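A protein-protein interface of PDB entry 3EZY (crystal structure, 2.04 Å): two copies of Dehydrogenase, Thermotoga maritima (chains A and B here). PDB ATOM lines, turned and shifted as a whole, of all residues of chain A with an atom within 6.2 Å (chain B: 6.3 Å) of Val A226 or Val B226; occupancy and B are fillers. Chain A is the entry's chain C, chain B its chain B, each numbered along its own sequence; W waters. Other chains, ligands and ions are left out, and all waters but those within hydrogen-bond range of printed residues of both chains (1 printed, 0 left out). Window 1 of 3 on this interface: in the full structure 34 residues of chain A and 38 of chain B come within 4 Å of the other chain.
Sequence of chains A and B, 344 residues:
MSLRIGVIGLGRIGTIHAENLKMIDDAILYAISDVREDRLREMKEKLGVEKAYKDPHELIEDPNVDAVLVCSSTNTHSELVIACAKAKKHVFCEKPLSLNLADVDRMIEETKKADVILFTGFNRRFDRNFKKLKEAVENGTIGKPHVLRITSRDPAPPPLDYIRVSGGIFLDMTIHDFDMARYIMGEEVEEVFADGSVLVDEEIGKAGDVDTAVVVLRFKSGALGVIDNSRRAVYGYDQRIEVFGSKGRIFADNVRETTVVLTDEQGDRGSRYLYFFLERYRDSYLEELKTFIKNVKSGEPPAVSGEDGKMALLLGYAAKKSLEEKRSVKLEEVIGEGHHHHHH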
ATOM      1  N   VAL A 147      -2.814   5.618  20.070  1.00  0.00           N
ATOM      2  CA  VAL A 147      -1.631   5.868  20.881  1.00  0.00           C
ATOM      3  C   VAL A 147      -2.011   6.572  22.170  1.00  0.00           C
ATOM      4  O   VAL A 147      -2.740   7.598  22.168  1.00  0.00           O
ATOM      5  CB  VAL A 147      -0.585   6.754  20.135  1.00  0.00           C
ATOM      6  CG1 VAL A 147       0.701   6.901  20.984  1.00  0.00           C
ATOM      7  CG2 VAL A 147      -0.239   6.135  18.776  1.00  0.00           C
ATOM      8  N   LEU A 148      -1.560   5.992  23.269  1.00  0.00           N
ATOM      9  CA  LEU A 148      -1.710   6.561  24.594  1.00  0.00           C
ATOM     10  C   LEU A 148      -0.347   7.090  25.018  1.00  0.00           C
ATOM     11  O   LEU A 148       0.653   6.384  24.829  1.00  0.00           O
ATOM     12  CB  LEU A 148      -2.152   5.472  25.587  1.00  0.00           C
ATOM     13  CG  LEU A 148      -2.026   5.833  27.070  1.00  0.00           C
ATOM     14  CD1 LEU A 148      -3.138   6.863  27.481  1.00  0.00           C
ATOM     15  CD2 LEU A 148      -2.055   4.509  27.943  1.00  0.00           C
ATOM     16  N   ARG A 149      -0.313   8.315  25.575  1.00  0.00           N
ATOM     17  CA  ARG A 149       0.855   8.905  26.233  1.00  0.00           C
ATOM     18  C   ARG A 149       0.515   9.224  27.682  1.00  0.00           C
ATOM     19  O   ARG A 149      -0.468   9.939  27.934  1.00  0.00           O
ATOM     20  CB  ARG A 149       1.243  10.252  25.591  1.00  0.00           C
ATOM     21  CG  ARG A 149       2.012  10.143  24.308  1.00  0.00           C
ATOM     22  CD  ARG A 149       3.460   9.719  24.599  1.00  0.00           C
ATOM     23  NE  ARG A 149       4.338   9.927  23.444  1.00  0.00           N
ATOM     24  CZ  ARG A 149       5.657   9.981  23.529  1.00  0.00           C
ATOM     25  NH1 ARG A 149       6.228   9.860  24.731  1.00  0.00           N
ATOM     26  NH2 ARG A 149       6.381  10.189  22.431  1.00  0.00           N
ATOM     27  N   ILE A 150       1.351   8.784  28.631  1.00  0.00           N
ATOM     28  CA  ILE A 150       1.172   9.170  30.035  1.00  0.00           C
ATOM     29  C   ILE A 150       2.524   9.660  30.488  1.00  0.00           C
ATOM     30  O   ILE A 150       3.510   8.929  30.325  1.00  0.00           O
ATOM     31  CB  ILE A 150       0.794   7.969  30.943  1.00  0.00           C
ATOM     32  CG1 ILE A 150      -0.572   7.396  30.559  1.00  0.00           C
ATOM     33  CG2 ILE A 150       0.812   8.364  32.432  1.00  0.00           C
ATOM     34  CD1 ILE A 150      -1.129   6.332  31.571  1.00  0.00           C
ATOM     35  N   THR A 151       2.596  10.863  31.052  1.00  0.00           N
ATOM     36  CA  THR A 151       3.829  11.316  31.745  1.00  0.00           C
ATOM     37  C   THR A 151       3.496  11.508  33.216  1.00  0.00           C
ATOM     38  O   THR A 151       2.510  12.197  33.527  1.00  0.00           O
ATOM     39  CB  THR A 151       4.342  12.676  31.204  1.00  0.00           C
ATOM     40  OG1 THR A 151       4.827  12.510  29.859  1.00  0.00           O
ATOM     41  CG2 THR A 151       5.473  13.243  32.109  1.00  0.00           C
ATOM     42  N   VAL A 214      11.098   4.724  31.014  1.00  0.00           N
ATOM     43  CA  VAL A 214      10.111   4.787  29.959  1.00  0.00           C
ATOM     44  C   VAL A 214       9.551   3.389  29.813  1.00  0.00           C
ATOM     45  O   VAL A 214      10.291   2.410  30.007  1.00  0.00           O
ATOM     46  CB  VAL A 214      10.773   5.237  28.676  1.00  0.00           C
ATOM     47  CG1 VAL A 214       9.877   4.941  27.516  1.00  0.00           C
ATOM     48  CG2 VAL A 214      11.183   6.779  28.795  1.00  0.00           C
ATOM     49  N   VAL A 215       8.259   3.262  29.528  1.00  0.00           N
ATOM     50  CA  VAL A 215       7.665   1.934  29.355  1.00  0.00           C
ATOM     51  C   VAL A 215       6.775   1.941  28.125  1.00  0.00           C
ATOM     52  O   VAL A 215       5.876   2.789  28.032  1.00  0.00           O
ATOM     53  CB  VAL A 215       6.823   1.543  30.599  1.00  0.00           C
ATOM     54  CG1 VAL A 215       6.353   0.114  30.483  1.00  0.00           C
ATOM     55  CG2 VAL A 215       7.640   1.656  31.802  1.00  0.00           C
ATOM     56  N   VAL A 216       6.996   1.022  27.174  1.00  0.00           N
ATOM     57  CA  VAL A 216       6.093   0.877  26.032  1.00  0.00           C
ATOM     58  C   VAL A 216       5.079  -0.224  26.251  1.00  0.00           C
ATOM     59  O   VAL A 216       5.432  -1.333  26.694  1.00  0.00           O
ATOM     60  CB  VAL A 216       6.831   0.568  24.685  1.00  0.00           C
ATOM     61  CG1 VAL A 216       5.800   0.336  23.525  1.00  0.00           C
ATOM     62  CG2 VAL A 216       7.801   1.643  24.365  1.00  0.00           C
ATOM     63  N   LEU A 217       3.818   0.064  25.923  1.00  0.00           N
ATOM     64  CA  LEU A 217       2.712  -0.874  26.094  1.00  0.00           C
ATOM     65  C   LEU A 217       2.148  -1.275  24.753  1.00  0.00           C
ATOM     66  O   LEU A 217       1.899  -0.421  23.891  1.00  0.00           O
ATOM     67  CB  LEU A 217       1.562  -0.234  26.934  1.00  0.00           C
ATOM     68  CG  LEU A 217       1.922   0.476  28.261  1.00  0.00           C
ATOM     69  CD1 LEU A 217       0.712   1.175  28.913  1.00  0.00           C
ATOM     70  CD2 LEU A 217       2.595  -0.452  29.236  1.00  0.00           C
ATOM     71  N   LEU A 224      -0.825   1.330  20.829  1.00  0.00           N
ATOM     72  CA  LEU A 224       0.436   1.396  21.559  1.00  0.00           C
ATOM     73  C   LEU A 224       0.410   2.468  22.652  1.00  0.00           C
ATOM     74  O   LEU A 224      -0.270   3.492  22.528  1.00  0.00           O
ATOM     75  CB  LEU A 224       1.611   1.676  20.582  1.00  0.00           C
ATOM     76  CG  LEU A 224       1.861   0.567  19.532  1.00  0.00           C
ATOM     77  CD1 LEU A 224       2.905   0.981  18.493  1.00  0.00           C
ATOM     78  CD2 LEU A 224       2.275  -0.745  20.188  1.00  0.00           C
ATOM     79  N   GLY A 225       1.106   2.226  23.748  1.00  0.00           N
ATOM     80  CA  GLY A 225       1.182   3.246  24.759  1.00  0.00           C
ATOM     81  C   GLY A 225       2.606   3.533  25.111  1.00  0.00           C
ATOM     82  O   GLY A 225       3.479   2.669  24.956  1.00  0.00           O
ATOM     83  N   VAL A 226       2.839   4.725  25.650  1.00  0.00           N
ATOM     84  CA  VAL A 226       4.140   5.077  26.164  1.00  0.00           C
ATOM     85  C   VAL A 226       3.990   5.809  27.507  1.00  0.00           C
ATOM     86  O   VAL A 226       3.386   6.888  27.551  1.00  0.00           O
ATOM     87  CB  VAL A 226       4.896   5.994  25.173  1.00  0.00           C
ATOM     88  CG1 VAL A 226       6.174   6.481  25.785  1.00  0.00           C
ATOM     89  CG2 VAL A 226       5.206   5.250  23.869  1.00  0.00           C
ATOM     90  N   ILE A 227       4.536   5.240  28.586  1.00  0.00           N
ATOM     91  CA  ILE A 227       4.622   5.928  29.879  1.00  0.00           C
ATOM     92  C   ILE A 227       6.051   6.418  30.166  1.00  0.00           C
ATOM     93  O   ILE A 227       6.983   5.640  30.027  1.00  0.00           O
ATOM     94  CB  ILE A 227       4.241   4.974  31.060  1.00  0.00           C
ATOM     95  CG1 ILE A 227       2.837   4.354  30.882  1.00  0.00           C
ATOM     96  CG2 ILE A 227       4.408   5.701  32.414  1.00  0.00           C
ATOM     97  CD1 ILE A 227       2.652   3.075  31.711  1.00  0.00           C
ATOM     98  N   ASP A 228       6.244   7.668  30.596  1.00  0.00           N
ATOM     99  CA  ASP A 228       7.544   8.046  31.158  1.00  0.00           C
ATOM    100  C   ASP A 228       7.405   8.583  32.578  1.00  0.00           C
ATOM    101  O   ASP A 228       6.392   9.248  32.904  1.00  0.00           O
ATOM    102  CB  ASP A 228       8.343   8.995  30.236  1.00  0.00           C
ATOM    103  CG  ASP A 228       7.736  10.400  30.144  1.00  0.00           C
ATOM    104  OD1 ASP A 228       8.349  11.331  30.732  1.00  0.00           O
ATOM    105  OD2 ASP A 228       6.663  10.570  29.512  1.00  0.00           O
ATOM    106  N   VAL B 147      14.891  13.339  29.610  1.00  0.00           N
ATOM    107  CA  VAL B 147      13.862  12.640  28.802  1.00  0.00           C
ATOM    108  C   VAL B 147      13.396  13.500  27.611  1.00  0.00           C
ATOM    109  O   VAL B 147      13.087  14.713  27.761  1.00  0.00           O
ATOM    110  CB  VAL B 147      12.599  12.285  29.605  1.00  0.00           C
ATOM    111  CG1 VAL B 147      11.611  11.554  28.701  1.00  0.00           C
ATOM    112  CG2 VAL B 147      12.911  11.398  30.853  1.00  0.00           C
ATOM    113  N   LEU B 148      13.418  12.901  26.436  1.00  0.00           N
ATOM    114  CA  LEU B 148      13.059  13.584  25.209  1.00  0.00           C
ATOM    115  C   LEU B 148      11.740  12.966  24.794  1.00  0.00           C
ATOM    116  O   LEU B 148      11.597  11.745  24.830  1.00  0.00           O
ATOM    117  CB  LEU B 148      14.075  13.309  24.088  1.00  0.00           C
ATOM    118  CG  LEU B 148      13.669  13.723  22.655  1.00  0.00           C
ATOM    119  CD1 LEU B 148      13.544  15.269  22.466  1.00  0.00           C
ATOM    120  CD2 LEU B 148      14.660  13.202  21.648  1.00  0.00           C
ATOM    121  N   ARG B 149      10.800  13.797  24.354  1.00  0.00           N
ATOM    122  CA  ARG B 149       9.571  13.298  23.738  1.00  0.00           C
ATOM    123  C   ARG B 149       9.414  13.983  22.392  1.00  0.00           C
ATOM    124  O   ARG B 149       9.445  15.229  22.312  1.00  0.00           O
ATOM    125  CB  ARG B 149       8.349  13.643  24.596  1.00  0.00           C
ATOM    126  CG  ARG B 149       7.061  13.187  23.977  1.00  0.00           C
ATOM    127  CD  ARG B 149       6.177  14.263  23.366  1.00  0.00           C
ATOM    128  NE  ARG B 149       4.881  13.753  22.888  1.00  0.00           N
ATOM    129  CZ  ARG B 149       3.717  13.823  23.562  1.00  0.00           C
ATOM    130  NH1 ARG B 149       3.659  14.360  24.800  1.00  0.00           N
ATOM    131  NH2 ARG B 149       2.598  13.315  23.000  1.00  0.00           N
ATOM    132  N   ILE B 150       9.240  13.178  21.348  1.00  0.00           N
ATOM    133  CA  ILE B 150       8.863  13.689  20.063  1.00  0.00           C
ATOM    134  C   ILE B 150       7.581  12.976  19.587  1.00  0.00           C
ATOM    135  O   ILE B 150       7.513  11.751  19.590  1.00  0.00           O
ATOM    136  CB  ILE B 150       9.993  13.443  19.032  1.00  0.00           C
ATOM    137  CG1 ILE B 150      11.206  14.286  19.382  1.00  0.00           C
ATOM    138  CG2 ILE B 150       9.525  13.734  17.647  1.00  0.00           C
ATOM    139  CD1 ILE B 150      12.379  14.060  18.443  1.00  0.00           C
ATOM    140  N   THR B 151       6.576  13.766  19.189  1.00  0.00           N
ATOM    141  CA  THR B 151       5.368  13.265  18.529  1.00  0.00           C
ATOM    142  C   THR B 151       5.355  13.860  17.091  1.00  0.00           C
ATOM    143  O   THR B 151       5.479  15.068  16.949  1.00  0.00           O
ATOM    144  CB  THR B 151       4.129  13.728  19.293  1.00  0.00           C
ATOM    145  OG1 THR B 151       4.045  13.024  20.540  1.00  0.00           O
ATOM    146  CG2 THR B 151       2.891  13.445  18.476  1.00  0.00           C
ATOM    147  N   VAL B 214       6.071   3.464  17.684  1.00  0.00           N
ATOM    148  CA  VAL B 214       6.779   4.071  18.799  1.00  0.00           C
ATOM    149  C   VAL B 214       8.261   3.631  18.800  1.00  0.00           C
ATOM    150  O   VAL B 214       8.596   2.482  18.427  1.00  0.00           O
ATOM    151  CB  VAL B 214       6.171   3.606  20.153  1.00  0.00           C
ATOM    152  CG1 VAL B 214       7.129   3.936  21.268  1.00  0.00           C
ATOM    153  CG2 VAL B 214       4.837   4.248  20.379  1.00  0.00           C
ATOM    154  N   VAL B 215       9.165   4.522  19.201  1.00  0.00           N
ATOM    155  CA  VAL B 215      10.574   4.150  19.163  1.00  0.00           C
ATOM    156  C   VAL B 215      11.181   4.709  20.407  1.00  0.00           C
ATOM    157  O   VAL B 215      11.059   5.921  20.659  1.00  0.00           O
ATOM    158  CB  VAL B 215      11.329   4.773  17.951  1.00  0.00           C
ATOM    159  CG1 VAL B 215      12.835   4.432  18.028  1.00  0.00           C
ATOM    160  CG2 VAL B 215      10.698   4.334  16.599  1.00  0.00           C
ATOM    161  N   VAL B 216      11.826   3.863  21.202  1.00  0.00           N
ATOM    162  CA  VAL B 216      12.534   4.341  22.360  1.00  0.00           C
ATOM    163  C   VAL B 216      14.021   4.500  22.050  1.00  0.00           C
ATOM    164  O   VAL B 216      14.639   3.629  21.430  1.00  0.00           O
ATOM    165  CB  VAL B 216      12.393   3.382  23.525  1.00  0.00           C
ATOM    166  CG1 VAL B 216      13.165   3.911  24.800  1.00  0.00           C
ATOM    167  CG2 VAL B 216      10.962   3.138  23.805  1.00  0.00           C
ATOM    168  N   LEU B 217      14.603   5.579  22.537  1.00  0.00           N
ATOM    169  CA  LEU B 217      16.002   5.887  22.273  1.00  0.00           C
ATOM    170  C   LEU B 217      16.782   5.917  23.571  1.00  0.00           C
ATOM    171  O   LEU B 217      16.346   6.519  24.545  1.00  0.00           O
ATOM    172  CB  LEU B 217      16.130   7.275  21.597  1.00  0.00           C
ATOM    173  CG  LEU B 217      15.328   7.558  20.314  1.00  0.00           C
ATOM    174  CD1 LEU B 217      15.575   9.008  19.864  1.00  0.00           C
ATOM    175  CD2 LEU B 217      15.692   6.593  19.198  1.00  0.00           C
ATOM    176  N   LEU B 224      16.896   9.238  28.093  1.00  0.00           N
ATOM    177  CA  LEU B 224      15.985   8.383  27.323  1.00  0.00           C
ATOM    178  C   LEU B 224      15.098   9.236  26.412  1.00  0.00           C
ATOM    179  O   LEU B 224      14.765  10.391  26.735  1.00  0.00           O
ATOM    180  CB  LEU B 224      15.140   7.533  28.298  1.00  0.00           C
ATOM    181  CG  LEU B 224      15.915   6.554  29.208  1.00  0.00           C
ATOM    182  CD1 LEU B 224      15.012   5.990  30.336  1.00  0.00           C
ATOM    183  CD2 LEU B 224      16.468   5.369  28.369  1.00  0.00           C
ATOM    184  N   GLY B 225      14.721   8.714  25.257  1.00  0.00           N
ATOM    185  CA  GLY B 225      13.772   9.453  24.402  1.00  0.00           C
ATOM    186  C   GLY B 225      12.675   8.562  23.856  1.00  0.00           C
ATOM    187  O   GLY B 225      12.838   7.334  23.757  1.00  0.00           O
ATOM    188  N   VAL B 226      11.539   9.150  23.494  1.00  0.00           N
ATOM    189  CA  VAL B 226      10.515   8.347  22.857  1.00  0.00           C
ATOM    190  C   VAL B 226       9.929   9.153  21.744  1.00  0.00           C
ATOM    191  O   VAL B 226       9.557  10.328  21.963  1.00  0.00           O
ATOM    192  CB  VAL B 226       9.381   7.933  23.826  1.00  0.00           C
ATOM    193  CG1 VAL B 226       8.538   6.775  23.190  1.00  0.00           C
ATOM    194  CG2 VAL B 226       9.954   7.451  25.168  1.00  0.00           C
ATOM    195  N   ILE B 227       9.851   8.532  20.561  1.00  0.00           N
ATOM    196  CA  ILE B 227       9.235   9.154  19.407  1.00  0.00           C
ATOM    197  C   ILE B 227       7.934   8.400  19.164  1.00  0.00           C
ATOM    198  O   ILE B 227       7.915   7.171  19.248  1.00  0.00           O
ATOM    199  CB  ILE B 227      10.092   8.949  18.126  1.00  0.00           C
ATOM    200  CG1 ILE B 227      11.512   9.510  18.272  1.00  0.00           C
ATOM    201  CG2 ILE B 227       9.354   9.501  16.878  1.00  0.00           C
ATOM    202  CD1 ILE B 227      12.466   8.997  17.179  1.00  0.00           C
ATOM    203  N   ASP B 228       6.841   9.083  18.862  1.00  0.00           N
ATOM    204  CA  ASP B 228       5.709   8.309  18.303  1.00  0.00           C
ATOM    205  C   ASP B 228       5.285   8.918  17.006  1.00  0.00           C
ATOM    206  O   ASP B 228       5.359  10.165  16.848  1.00  0.00           O
ATOM    207  CB  ASP B 228       4.536   8.106  19.299  1.00  0.00           C
ATOM    208  CG  ASP B 228       3.839   9.425  19.671  1.00  0.00           C
ATOM    209  OD1 ASP B 228       2.703   9.661  19.176  1.00  0.00           O
ATOM    210  OD2 ASP B 228       4.448  10.221  20.435  1.00  0.00           O
HETATM  211  O   HOH W   1       5.370  14.220  27.417  1.00  0.00           O
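Hydrophobic or aromatic side chains of chain B within 4 Å of the printed part of chain A: Val B147, Val B214, Val B216 and Val B226. Along chain B the printed residues that touch a printed residue of chain A span positions 147 to 228. Printed residues of chain A that touch a printed residue of chain B: Val A147, Arg A149, Val A214, Val A216, Val A226 and Asp A228. Among the printed residues, 11 pairs touch across the chains.
OG1 of Thr B151 sits at hydrogen-bond distance from NE of Arg B149, at 2.6 Å. The backbone NH of Asp B228 lies within hydrogen-bond range of the backbone carbonyl oxygen of Ile B150 (2.8 Å). The backbone NH (N) of Val A226 is in hydrogen-bond range of the backbone carbonyl oxygen (O) of Leu A148. The backbone NH (N) of Ile A150 is in hydrogen-bond range of the backbone carbonyl oxygen (O) of Val A226. The backbone NH of Asp A228 lies within hydrogen-bond range of the backbone carbonyl oxygen of Ile A150 (3.0 Å). OG1 of Thr A151 lies within hydrogen-bond range of OD2 of Asp A228, at 2.7 Å.
Among the printed residues, merely in contact across the chains: Val A147 with Asp B228, Arg A149 with Arg B149, Val A214 with Val B226, Val A216 with Val B214, Val A216 with Val B216, Val A226 with Val B214, Val A226 with Val B226 and Asp A228 with Val B147.
Of the printed residues of chain A, Val B226 touches Arg A149, Val A214 and Val A226. Printed residues of chain A within 4 Å of Val B147: Asp A228 (3.8 Å). Of the printed residues of chain A, Val B214 touches Val A216 (3.9 Å) and Val A226 (3.5 Å). Of the printed residues of chain A, Ile B150 touches Arg A149. Of the printed residues of chain A, Val B216 touches Val A216 (3.5 Å). Leu B217 touches none of the printed residues of chain A. Val B215 touches none of the printed residues of chain A. The nearest residue of chain B that does not touch Val A226 is Asp B228 (5.4 Å).
The backbone carbonyl oxygen of Ile B150 is in hydrogen-bond range of the guanidinium group of Arg A149 (3.4 Å). The backbone carbonyl oxygen of Val B226 sits at hydrogen-bond distance from the guanidinium group of Arg A149, at 3.2 Å. The side-chain carboxylate (OD2) of Asp B228 is in salt-bridge range of the guanidinium group (NH2) of Arg A149 (2.8 Å).
Water W1 lies within hydrogen-bond range of the side-chain hydroxyl (OG1) of Thr A151 and the guanidinium group (NH1) of Arg B149.
Val A147 touches Asp B228, and with the chains exchanged Asp A228 touches Val B147. Arg B149 touches its own counterpart, Arg A149. Val A214 touches Val B226, and with the chains exchanged Val A226 touches Val B214. Val B226 touches its own counterpart, Val A226. Of the 11 pairs that touch across the chains among the printed residues, 7 have their exchanged pair printed and touching as well.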
